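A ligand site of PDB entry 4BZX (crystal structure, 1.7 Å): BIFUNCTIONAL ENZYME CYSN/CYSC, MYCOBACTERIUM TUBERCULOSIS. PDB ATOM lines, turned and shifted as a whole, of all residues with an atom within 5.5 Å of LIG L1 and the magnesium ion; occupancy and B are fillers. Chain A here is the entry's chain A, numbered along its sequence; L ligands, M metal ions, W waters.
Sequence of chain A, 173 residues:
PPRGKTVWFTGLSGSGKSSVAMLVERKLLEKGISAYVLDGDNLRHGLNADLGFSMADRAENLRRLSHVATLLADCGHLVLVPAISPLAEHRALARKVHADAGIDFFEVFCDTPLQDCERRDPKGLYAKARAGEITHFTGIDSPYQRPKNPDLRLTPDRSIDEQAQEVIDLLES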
ATOM      1  N   GLY A  11      -4.326 -23.719  19.533  1.00  0.00           N
ATOM      2  CA  GLY A  11      -4.280 -22.840  20.688  1.00  0.00           C
ATOM      3  C   GLY A  11      -4.334 -21.403  20.257  1.00  0.00           C
ATOM      4  O   GLY A  11      -4.110 -21.062  19.089  1.00  0.00           O
ATOM      5  N   LEU A  12      -4.558 -20.553  21.252  1.00  0.00           N
ATOM      6  CA  LEU A  12      -4.601 -19.118  21.079  1.00  0.00           C
ATOM      7  C   LEU A  12      -3.324 -18.569  20.444  1.00  0.00           C
ATOM      8  O   LEU A  12      -2.230 -19.127  20.539  1.00  0.00           O
ATOM      9  CB  LEU A  12      -4.867 -18.405  22.408  1.00  0.00           C
ATOM     10  CG  LEU A  12      -6.207 -18.686  23.111  1.00  0.00           C
ATOM     11  CD1 LEU A  12      -6.254 -17.991  24.433  1.00  0.00           C
ATOM     12  CD2 LEU A  12      -7.383 -18.237  22.269  1.00  0.00           C
ATOM     13  N   SER A  13      -3.483 -17.422  19.787  1.00  0.00           N
ATOM     14  CA  SER A  13      -2.334 -16.666  19.409  1.00  0.00           C
ATOM     15  C   SER A  13      -1.467 -16.345  20.622  1.00  0.00           C
ATOM     16  O   SER A  13      -1.952 -15.946  21.660  1.00  0.00           O
ATOM     17  CB  SER A  13      -2.738 -15.398  18.674  1.00  0.00           C
ATOM     18  OG  SER A  13      -1.588 -14.699  18.274  1.00  0.00           O
ATOM     19  N   GLY A  14      -0.148 -16.591  20.500  1.00  0.00           N
ATOM     20  CA  GLY A  14       0.775 -16.361  21.609  1.00  0.00           C
ATOM     21  C   GLY A  14       0.884 -17.485  22.615  1.00  0.00           C
ATOM     22  O   GLY A  14       1.645 -17.333  23.596  1.00  0.00           O
ATOM     23  N   SER A  15       0.237 -18.619  22.338  1.00  0.00           N
ATOM     24  CA  SER A  15       0.250 -19.779  23.271  1.00  0.00           C
ATOM     25  C   SER A  15       1.542 -20.630  23.213  1.00  0.00           C
ATOM     26  O   SER A  15       1.795 -21.400  24.128  1.00  0.00           O
ATOM     27  CB  SER A  15      -0.987 -20.631  23.126  1.00  0.00           C
ATOM     28  OG  SER A  15      -1.075 -21.216  21.810  1.00  0.00           O
ATOM     29  N   GLY A  16       2.380 -20.428  22.178  1.00  0.00           N
ATOM     30  CA  GLY A  16       3.666 -21.128  22.033  1.00  0.00           C
ATOM     31  C   GLY A  16       3.728 -22.201  20.976  1.00  0.00           C
ATOM     32  O   GLY A  16       4.673 -23.015  20.949  1.00  0.00           O
ATOM     33  N   LYS A  17       2.724 -22.243  20.122  1.00  0.00           N
ATOM     34  CA  LYS A  17       2.659 -23.327  19.119  1.00  0.00           C
ATOM     35  C   LYS A  17       3.901 -23.386  18.241  1.00  0.00           C
ATOM     36  O   LYS A  17       4.509 -24.452  18.075  1.00  0.00           O
ATOM     37  CB  LYS A  17       1.420 -23.167  18.234  1.00  0.00           C
ATOM     38  CG  LYS A  17       0.091 -23.185  18.968  1.00  0.00           C
ATOM     39  CD  LYS A  17      -1.128 -22.984  18.058  1.00  0.00           C
ATOM     40  CE  LYS A  17      -1.127 -21.698  17.244  1.00  0.00           C
ATOM     41  NZ  LYS A  17      -1.247 -20.531  18.170  1.00  0.00           N
ATOM     42  N   SER A  18       4.223 -22.276  17.622  1.00  0.00           N
ATOM     43  CA  SER A  18       5.348 -22.165  16.674  1.00  0.00           C
ATOM     44  C   SER A  18       6.688 -22.393  17.364  1.00  0.00           C
ATOM     45  O   SER A  18       7.562 -23.139  16.845  1.00  0.00           O
ATOM     46  CB  SER A  18       5.411 -20.792  15.969  1.00  0.00           C
ATOM     47  OG  SER A  18       4.252 -20.600  15.162  1.00  0.00           O
ATOM     48  N   SER A  19       6.835 -21.890  18.587  1.00  0.00           N
ATOM     49  CA  SER A  19       8.068 -22.096  19.337  1.00  0.00           C
ATOM     50  C   SER A  19       8.354 -23.543  19.663  1.00  0.00           C
ATOM     51  O   SER A  19       9.496 -24.030  19.433  1.00  0.00           O
ATOM     52  CB  SER A  19       8.023 -21.285  20.675  1.00  0.00           C
ATOM     53  OG  SER A  19       7.999 -19.928  20.319  1.00  0.00           O
ATOM     54  N   VAL A  20       7.327 -24.223  20.192  1.00  0.00           N
ATOM     55  CA  VAL A  20       7.424 -25.623  20.459  1.00  0.00           C
ATOM     56  C   VAL A  20       7.629 -26.429  19.196  1.00  0.00           C
ATOM     57  O   VAL A  20       8.549 -27.277  19.183  1.00  0.00           O
ATOM     58  CB  VAL A  20       6.216 -26.158  21.242  1.00  0.00           C
ATOM     59  CG1 VAL A  20       6.388 -27.645  21.450  1.00  0.00           C
ATOM     60  CG2 VAL A  20       6.139 -25.419  22.560  1.00  0.00           C
ATOM     61  N   ASP A  39       3.919 -24.077   9.237  1.00  0.00           N
ATOM     62  CA  ASP A  39       3.424 -23.046  10.182  1.00  0.00           C
ATOM     63  C   ASP A  39       2.344 -22.222   9.527  1.00  0.00           C
ATOM     64  O   ASP A  39       2.575 -21.648   8.440  1.00  0.00           O
ATOM     65  CB  ASP A  39       4.620 -22.201  10.594  1.00  0.00           C
ATOM     66  CG  ASP A  39       4.297 -21.132  11.668  1.00  0.00           C
ATOM     67  OD1 ASP A  39       3.539 -20.195  11.390  1.00  0.00           O
ATOM     68  OD2 ASP A  39       4.865 -21.222  12.754  1.00  0.00           O
ATOM     69  N   ASP A  41       1.093 -19.249  10.066  1.00  0.00           N
ATOM     70  CA  ASP A  41       1.488 -17.906   9.695  1.00  0.00           C
ATOM     71  C   ASP A  41       2.396 -17.871   8.464  1.00  0.00           C
ATOM     72  O   ASP A  41       2.261 -16.989   7.578  1.00  0.00           O
ATOM     73  CB  ASP A  41       2.185 -17.238  10.916  1.00  0.00           C
ATOM     74  CG  ASP A  41       2.513 -15.777  10.678  1.00  0.00           C
ATOM     75  OD1 ASP A  41       1.619 -14.968  10.469  1.00  0.00           O
ATOM     76  OD2 ASP A  41       3.680 -15.425  10.708  1.00  0.00           O
ATOM     77  N   PRO A  82       1.796 -25.922  13.524  1.00  0.00           N
ATOM     78  CA  PRO A  82       1.327 -24.915  14.443  1.00  0.00           C
ATOM     79  C   PRO A  82       0.371 -23.964  13.767  1.00  0.00           C
ATOM     80  O   PRO A  82       0.782 -23.156  12.889  1.00  0.00           O
ATOM     81  CB  PRO A  82       2.600 -24.255  14.884  1.00  0.00           C
ATOM     82  CG  PRO A  82       3.479 -24.342  13.695  1.00  0.00           C
ATOM     83  CD  PRO A  82       3.225 -25.670  13.155  1.00  0.00           C
ATOM     84  N   ILE A  84      -3.639 -21.961  14.659  1.00  0.00           N
ATOM     85  CA  ILE A  84      -4.587 -21.753  15.736  1.00  0.00           C
ATOM     86  C   ILE A  84      -5.673 -22.831  15.799  1.00  0.00           C
ATOM     87  O   ILE A  84      -5.952 -23.429  16.854  1.00  0.00           O
ATOM     88  CB  ILE A  84      -5.184 -20.303  15.653  1.00  0.00           C
ATOM     89  CG1 ILE A  84      -4.125 -19.284  16.052  1.00  0.00           C
ATOM     90  CG2 ILE A  84      -6.424 -20.171  16.585  1.00  0.00           C
ATOM     91  CD1 ILE A  84      -4.616 -17.872  15.785  1.00  0.00           C
ATOM     92  N   ARG A 120       2.027 -11.720  27.174  1.00  0.00           N
ATOM     93  CA  ARG A 120       3.212 -11.913  26.320  1.00  0.00           C
ATOM     94  C   ARG A 120       3.174 -10.941  25.171  1.00  0.00           C
ATOM     95  O   ARG A 120       4.062 -10.092  25.018  1.00  0.00           O
ATOM     96  CB  ARG A 120       3.258 -13.317  25.728  1.00  0.00           C
ATOM     97  CG  ARG A 120       3.510 -14.434  26.712  1.00  0.00           C
ATOM     98  CD  ARG A 120       3.131 -15.781  26.187  1.00  0.00           C
ATOM     99  NE  ARG A 120       3.527 -16.818  27.143  1.00  0.00           N
ATOM    100  CZ  ARG A 120       3.313 -18.106  26.992  1.00  0.00           C
ATOM    101  NH1 ARG A 120       2.698 -18.575  25.917  1.00  0.00           N
ATOM    102  NH2 ARG A 120       3.724 -18.980  27.926  1.00  0.00           N
ATOM    103  N   PRO A 122       3.546 -11.029  21.709  1.00  0.00           N
ATOM    104  CA  PRO A 122       4.797 -10.861  20.882  1.00  0.00           C
ATOM    105  C   PRO A 122       4.735 -10.134  19.566  1.00  0.00           C
ATOM    106  O   PRO A 122       5.719  -9.534  19.178  1.00  0.00           O
ATOM    107  CB  PRO A 122       5.274 -12.295  20.614  1.00  0.00           C
ATOM    108  CG  PRO A 122       4.247 -13.184  21.176  1.00  0.00           C
ATOM    109  CD  PRO A 122       3.192 -12.444  21.923  1.00  0.00           C
ATOM    110  N   LYS A 123       3.587 -10.090  18.889  1.00  0.00           N
ATOM    111  CA  LYS A 123       3.436  -9.330  17.648  1.00  0.00           C
ATOM    112  C   LYS A 123       2.527  -8.102  17.788  1.00  0.00           C
ATOM    113  O   LYS A 123       2.220  -7.416  16.798  1.00  0.00           O
ATOM    114  CB  LYS A 123       2.850 -10.263  16.583  1.00  0.00           C
ATOM    115  CG  LYS A 123       3.689 -11.498  16.326  1.00  0.00           C
ATOM    116  CD  LYS A 123       2.986 -12.483  15.379  1.00  0.00           C
ATOM    117  CE  LYS A 123       3.360 -13.912  15.754  1.00  0.00           C
ATOM    118  NZ  LYS A 123       2.835 -15.011  14.880  1.00  0.00           N
ATOM    119  N   LEU A 125      -0.556  -7.938  18.471  1.00  0.00           N
ATOM    120  CA  LEU A 125      -1.889  -8.155  17.910  1.00  0.00           C
ATOM    121  C   LEU A 125      -2.988  -8.058  18.942  1.00  0.00           C
ATOM    122  O   LEU A 125      -4.063  -7.570  18.623  1.00  0.00           O
ATOM    123  CB  LEU A 125      -1.954  -9.540  17.265  1.00  0.00           C
ATOM    124  CG  LEU A 125      -1.081  -9.657  16.002  1.00  0.00           C
ATOM    125  CD1 LEU A 125      -1.192 -11.057  15.418  1.00  0.00           C
ATOM    126  CD2 LEU A 125      -1.440  -8.635  14.992  1.00  0.00           C
ATOM    127  N   THR A 155       1.291 -26.775  29.005  1.00  0.00           N
ATOM    128  CA  THR A 155       0.929 -25.644  29.859  1.00  0.00           C
ATOM    129  C   THR A 155       2.152 -24.809  30.153  1.00  0.00           C
ATOM    130  O   THR A 155       3.278 -25.282  30.115  1.00  0.00           O
ATOM    131  CB  THR A 155       0.347 -26.152  31.171  1.00  0.00           C
ATOM    132  OG1 THR A 155       1.272 -27.030  31.813  1.00  0.00           O
ATOM    133  CG2 THR A 155      -0.935 -26.970  30.927  1.00  0.00           C
ATOM    134  N   PRO A 156       1.950 -23.576  30.573  1.00  0.00           N
ATOM    135  CA  PRO A 156       3.185 -22.855  30.784  1.00  0.00           C
ATOM    136  C   PRO A 156       3.886 -23.153  32.105  1.00  0.00           C
ATOM    137  O   PRO A 156       4.320 -22.269  32.758  1.00  0.00           O
ATOM    138  CB  PRO A 156       2.754 -21.385  30.664  1.00  0.00           C
ATOM    139  CG  PRO A 156       1.263 -21.369  30.886  1.00  0.00           C
ATOM    140  CD  PRO A 156       0.751 -22.735  30.619  1.00  0.00           C
ATOM    141  N   ARG A 158       6.740 -25.187  32.085  1.00  0.00           N
ATOM    142  CA  ARG A 158       8.183 -25.509  31.873  1.00  0.00           C
ATOM    143  C   ARG A 158       8.789 -24.837  30.633  1.00  0.00           C
ATOM    144  O   ARG A 158       8.136 -24.067  30.034  1.00  0.00           O
ATOM    145  CB  ARG A 158       8.442 -27.030  31.884  1.00  0.00           C
ATOM    146  CG  ARG A 158       7.866 -27.687  30.637  1.00  0.00           C
ATOM    147  CD  ARG A 158       7.791 -29.211  30.793  1.00  0.00           C
ATOM    148  NE  ARG A 158       6.671 -29.568  31.682  1.00  0.00           N
ATOM    149  CZ  ARG A 158       6.316 -30.809  32.004  1.00  0.00           C
ATOM    150  NH1 ARG A 158       6.977 -31.845  31.522  1.00  0.00           N
ATOM    151  NH2 ARG A 158       5.266 -30.978  32.791  1.00  0.00           N
ATOM    152  N   SER A 159      10.111 -24.996  30.412  1.00  0.00           N
ATOM    153  CA  SER A 159      10.718 -24.279  29.327  1.00  0.00           C
ATOM    154  C   SER A 159      10.143 -24.792  28.004  1.00  0.00           C
ATOM    155  O   SER A 159       9.534 -25.874  27.910  1.00  0.00           O
ATOM    156  CB  SER A 159      12.241 -24.424  29.322  1.00  0.00           C
ATOM    157  OG  SER A 159      12.630 -25.732  28.999  1.00  0.00           O
ATOM    158  N   ILE A 160      10.319 -23.977  26.975  1.00  0.00           N
ATOM    159  CA  ILE A 160       9.960 -24.445  25.637  1.00  0.00           C
ATOM    160  C   ILE A 160      10.733 -25.745  25.374  1.00  0.00           C
ATOM    161  O   ILE A 160      10.198 -26.650  24.730  1.00  0.00           O
ATOM    162  CB  ILE A 160      10.280 -23.354  24.628  1.00  0.00           C
ATOM    163  CG1 ILE A 160       9.430 -22.127  24.975  1.00  0.00           C
ATOM    164  CG2 ILE A 160      10.048 -23.833  23.224  1.00  0.00           C
ATOM    165  CD1 ILE A 160       9.545 -21.028  23.985  1.00  0.00           C
ATOM    166  N   GLN A 163       8.893 -28.580  26.915  1.00  0.00           N
ATOM    167  CA  GLN A 163       7.652 -28.794  26.200  1.00  0.00           C
ATOM    168  C   GLN A 163       7.930 -29.570  24.912  1.00  0.00           C
ATOM    169  O   GLN A 163       7.170 -30.475  24.559  1.00  0.00           O
ATOM    170  CB  GLN A 163       6.922 -27.497  25.889  1.00  0.00           C
ATOM    171  CG  GLN A 163       6.376 -26.871  27.157  1.00  0.00           C
ATOM    172  CD  GLN A 163       5.693 -25.571  26.866  1.00  0.00           C
ATOM    173  OE1 GLN A 163       6.022 -24.911  25.895  1.00  0.00           O
ATOM    174  NE2 GLN A 163       4.738 -25.200  27.713  1.00  0.00           N
HETATM  175  P1  LIG L   1       0.521 -17.269  16.854  1.00  0.00           P
HETATM  176  O1  LIG L   1       0.172 -15.823  16.996  1.00  0.00           O
HETATM  177  O2  LIG L   1       1.531 -17.464  15.749  1.00  0.00           O
HETATM  178  O3  LIG L   1      -0.728 -18.232  16.632  1.00  0.00           O
HETATM  179  P2  LIG L   1       2.060 -19.064  18.695  1.00  0.00           P
HETATM  180  O4  LIG L   1       1.059 -19.953  19.447  1.00  0.00           O
HETATM  181  O5  LIG L   1       2.803 -19.669  17.551  1.00  0.00           O
HETATM  182  N1  LIG L   1       1.398 -17.645  18.260  1.00  0.00           N
HETATM  183  P3  LIG L   1       4.711 -18.366  19.660  1.00  0.00           P
HETATM  184  O6  LIG L   1       4.997 -17.340  18.600  1.00  0.00           O
HETATM  185  O7  LIG L   1       5.369 -19.696  19.515  1.00  0.00           O
HETATM  186  O8  LIG L   1       3.134 -18.505  19.848  1.00  0.00           O
HETATM  187  O9  LIG L   1       5.018 -17.848  21.193  1.00  0.00           O
HETATM  188  C1  LIG L   1       4.563 -16.674  21.783  1.00  0.00           C
HETATM  189  C2  LIG L   1       5.565 -16.391  22.922  1.00  0.00           C
HETATM  190  O10 LIG L   1       5.249 -17.141  24.025  1.00  0.00           O
HETATM  191  C3  LIG L   1       6.974 -16.779  22.516  1.00  0.00           C
HETATM  192  O11 LIG L   1       7.673 -15.567  22.203  1.00  0.00           O
HETATM  193  C4  LIG L   1       7.554 -17.480  23.696  1.00  0.00           C
HETATM  194  O12 LIG L   1       8.654 -16.726  24.165  1.00  0.00           O
HETATM  195  C5  LIG L   1       6.469 -17.495  24.706  1.00  0.00           C
HETATM  196  N2  LIG L   1       6.430 -18.843  25.243  1.00  0.00           N
HETATM  197  C6  LIG L   1       5.789 -19.906  24.664  1.00  0.00           C
HETATM  198  N3  LIG L   1       5.924 -21.020  25.429  1.00  0.00           N
HETATM  199  C7  LIG L   1       6.683 -20.665  26.499  1.00  0.00           C
HETATM  200  C8  LIG L   1       7.205 -21.333  27.708  1.00  0.00           C
HETATM  201  N4  LIG L   1       6.955 -22.641  27.886  1.00  0.00           N
HETATM  202  N5  LIG L   1       7.936 -20.596  28.602  1.00  0.00           N
HETATM  203  C9  LIG L   1       8.204 -19.285  28.407  1.00  0.00           C
HETATM  204  N6  LIG L   1       7.745 -18.609  27.344  1.00  0.00           N
HETATM  205  C10 LIG L   1       7.005 -19.233  26.381  1.00  0.00           C
HETATM  206  S1  LG2 L   2      -6.217 -20.306  11.677  1.00  0.00           S
HETATM  207  O1  LG2 L   2      -5.757 -21.578  12.157  1.00  0.00           O
HETATM  208  O2  LG2 L   2      -7.313 -19.748  12.449  1.00  0.00           O
HETATM  209  O3  LG2 L   2      -6.529 -20.281  10.223  1.00  0.00           O
HETATM  210  P1  LG2 L   2      -3.446 -19.454  11.557  1.00  0.00           P
HETATM  211  O4  LG2 L   2      -3.353 -19.909  10.130  1.00  0.00           O
HETATM  212  O5  LG2 L   2      -2.725 -20.220  12.590  1.00  0.00           O
HETATM  213  O6  LG2 L   2      -5.037 -19.285  11.886  1.00  0.00           O
HETATM  214  O7  LG2 L   2      -2.996 -17.916  11.531  1.00  0.00           O
HETATM  215  C1  LG2 L   2      -2.857 -17.291  12.778  1.00  0.00           C
HETATM  216  C2  LG2 L   2      -1.695 -16.299  12.585  1.00  0.00           C
HETATM  217  O8  LG2 L   2      -2.174 -15.053  12.048  1.00  0.00           O
HETATM  218  C3  LG2 L   2      -1.067 -16.064  13.929  1.00  0.00           C
HETATM  219  O9  LG2 L   2       0.362 -16.114  13.724  1.00  0.00           O
HETATM  220  C4  LG2 L   2      -1.586 -14.724  14.277  1.00  0.00           C
HETATM  221  O10 LG2 L   2      -0.517 -14.077  14.993  1.00  0.00           O
HETATM  222  C5  LG2 L   2      -1.986 -13.973  13.035  1.00  0.00           C
HETATM  223  N1  LG2 L   2      -3.280 -13.319  12.922  1.00  0.00           N
HETATM  224  C6  LG2 L   2      -3.523 -12.169  12.206  1.00  0.00           C
HETATM  225  N2  LG2 L   2      -4.802 -11.836  12.228  1.00  0.00           N
HETATM  226  C7  LG2 L   2      -5.413 -12.773  12.998  1.00  0.00           C
HETATM  227  C8  LG2 L   2      -6.777 -12.924  13.445  1.00  0.00           C
HETATM  228  N3  LG2 L   2      -7.722 -12.048  13.034  1.00  0.00           N
HETATM  229  N4  LG2 L   2      -7.031 -13.997  14.233  1.00  0.00           N
HETATM  230  C9  LG2 L   2      -6.073 -14.827  14.608  1.00  0.00           C
HETATM  231  N5  LG2 L   2      -4.762 -14.729  14.250  1.00  0.00           N
HETATM  232  C10 LG2 L   2      -4.422 -13.719  13.437  1.00  0.00           C
HETATM  233 MG    MG M   1       2.861 -19.052  15.582  1.00  0.00          MG
HETATM  234  O   HOH W   1       1.589 -20.429  14.778  1.00  0.00           O
HETATM  235  O   HOH W   2       8.582 -20.781  30.958  1.00  0.00           O
HETATM  236  O   HOH W   3       3.254 -22.068  27.126  1.00  0.00           O
HETATM  237  O   HOH W   4       2.548 -15.164  18.453  1.00  0.00           O
HETATM  238  O   HOH W   5       4.429 -17.724  16.128  1.00  0.00           O
HETATM  239  O   HOH W   6       3.311 -18.440  13.581  1.00  0.00           O
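The backbone NH (N) of Ser 18 is in hydrogen-bond range of an oxygen (O7) of LIG L1 (3.4 Å). An oxygen (O4) of LIG L1 is in hydrogen-bond range of the backbone NH (N) of Ser 15, at 3.3 Å. The side-chain hydroxyl (OG) of Ser 19 is in hydrogen-bond range of an oxygen (O7) of LIG L1 (2.8 Å). The backbone carbonyl oxygen (O) of Arg 158 is in hydrogen-bond range of a nitrogen (N4) of LIG L1 (2.8 Å). NH1 of Arg 120 sits close to O10 of LIG L1 (3.5 Å). The backbone NH of Ile 84 lies within hydrogen-bond range of an oxygen (O5) of LG2 L2. O1 of LIG L1 is in hydrogen-bond range of OG of Ser 13. The side-chain hydroxyl (OG) of Ser 15 is in hydrogen-bond range of an oxygen (O4) of LIG L1 (3.4 Å). N4 of LIG L1 is in hydrogen-bond range of OE1 of Gln 163 (3.2 Å). NZ of Lys 17 is in salt-bridge range of O4 of LIG L1 (2.7 Å). The side-chain amino group (NZ) of Lys 123 lies within hydrogen-bond range of an oxygen (O9) of LG2 L2 (2.9 Å). N of Gly 16 is in hydrogen-bond range of O4 of LIG L1 (3.1 Å). An oxygen (O4) of LIG L1 lies within hydrogen-bond range of the backbone NH of Lys 17. N of Ser 19 sits at hydrogen-bond distance from O7 of LIG L1. The side-chain amino group of Lys 123 lies within salt-bridge range of an oxygen (O1) of LIG L1, 3.5 Å away.
O1 of LIG L1 is in hydrogen-bond range of O10 of LG2 L2 (2.7 Å).
O of Ser 15 lies within hydrogen-bond range of NH1 of Arg 120 (3.5 Å). The side-chain hydroxyl of Ser 18 lies close to the side-chain carboxylate of Asp 39 (2.6 Å). O of Gly 14 is in hydrogen-bond range of NH1 of Arg 120 (2.8 Å). O of Ile 84 is in hydrogen-bond range of N of Gly 11, at 3.1 Å. The backbone carbonyl oxygen (O) of Thr 155 sits at hydrogen-bond distance from the side-chain amide nitrogen (NE2) of Gln 163, at 2.8 Å. The side-chain amino group of Lys 17 is in hydrogen-bond range of the backbone carbonyl oxygen of Leu 12 (2.9 Å). NZ of Lys 17 lies within hydrogen-bond range of O of Gly 11 (3.1 Å). O of Leu 12 sits at hydrogen-bond distance from OG of Ser 15, 2.7 Å away.
The backbone NH (N) of Gly 14 lies close to a nitrogen (N1) of LIG L1. Merely in contact with LIG L1: Ile 160, Pro 122, Leu 12, Ile 84 and Ser 159. Hydrophobic or aromatic side chains within 4 Å of LIG L1: Ile 84, Pro 122 and Ile 160. 16 residues have an atom within 4 Å of LIG L1: Leu 12, Ser 13, Gly 14, Ser 15, Gly 16, Lys 17, Ser 18, Ser 19, Ile 84, Arg 120, Pro 122, Lys 123, Arg 158, Ser 159, Ile 160 and Gln 163.
The nearest printed residue that does not touch the magnesium ion is Asp 39 (4.1 Å).
The magnesium ion is bound by water W1, O5 of LIG L1, O2 of LIG L1, OG of Ser 18, water W5 and water W6. The magnesium ion has six donor atoms within binding distance.
Water W5 bridges O6 of LIG L1 (2.6 Å) and NZ of Lys 123 (3.4 Å). Water W2 lies within hydrogen-bond range of a nitrogen (N5) of LIG L1 (2.4 Å) and the backbone carbonyl oxygen (O) of Arg 158 (3.4 Å). Water W3 lies within hydrogen-bond range of NH2 of Arg 120 (3.2 Å), N3 of LIG L1 (3.3 Å) and O of Ser 15 (3.4 Å).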
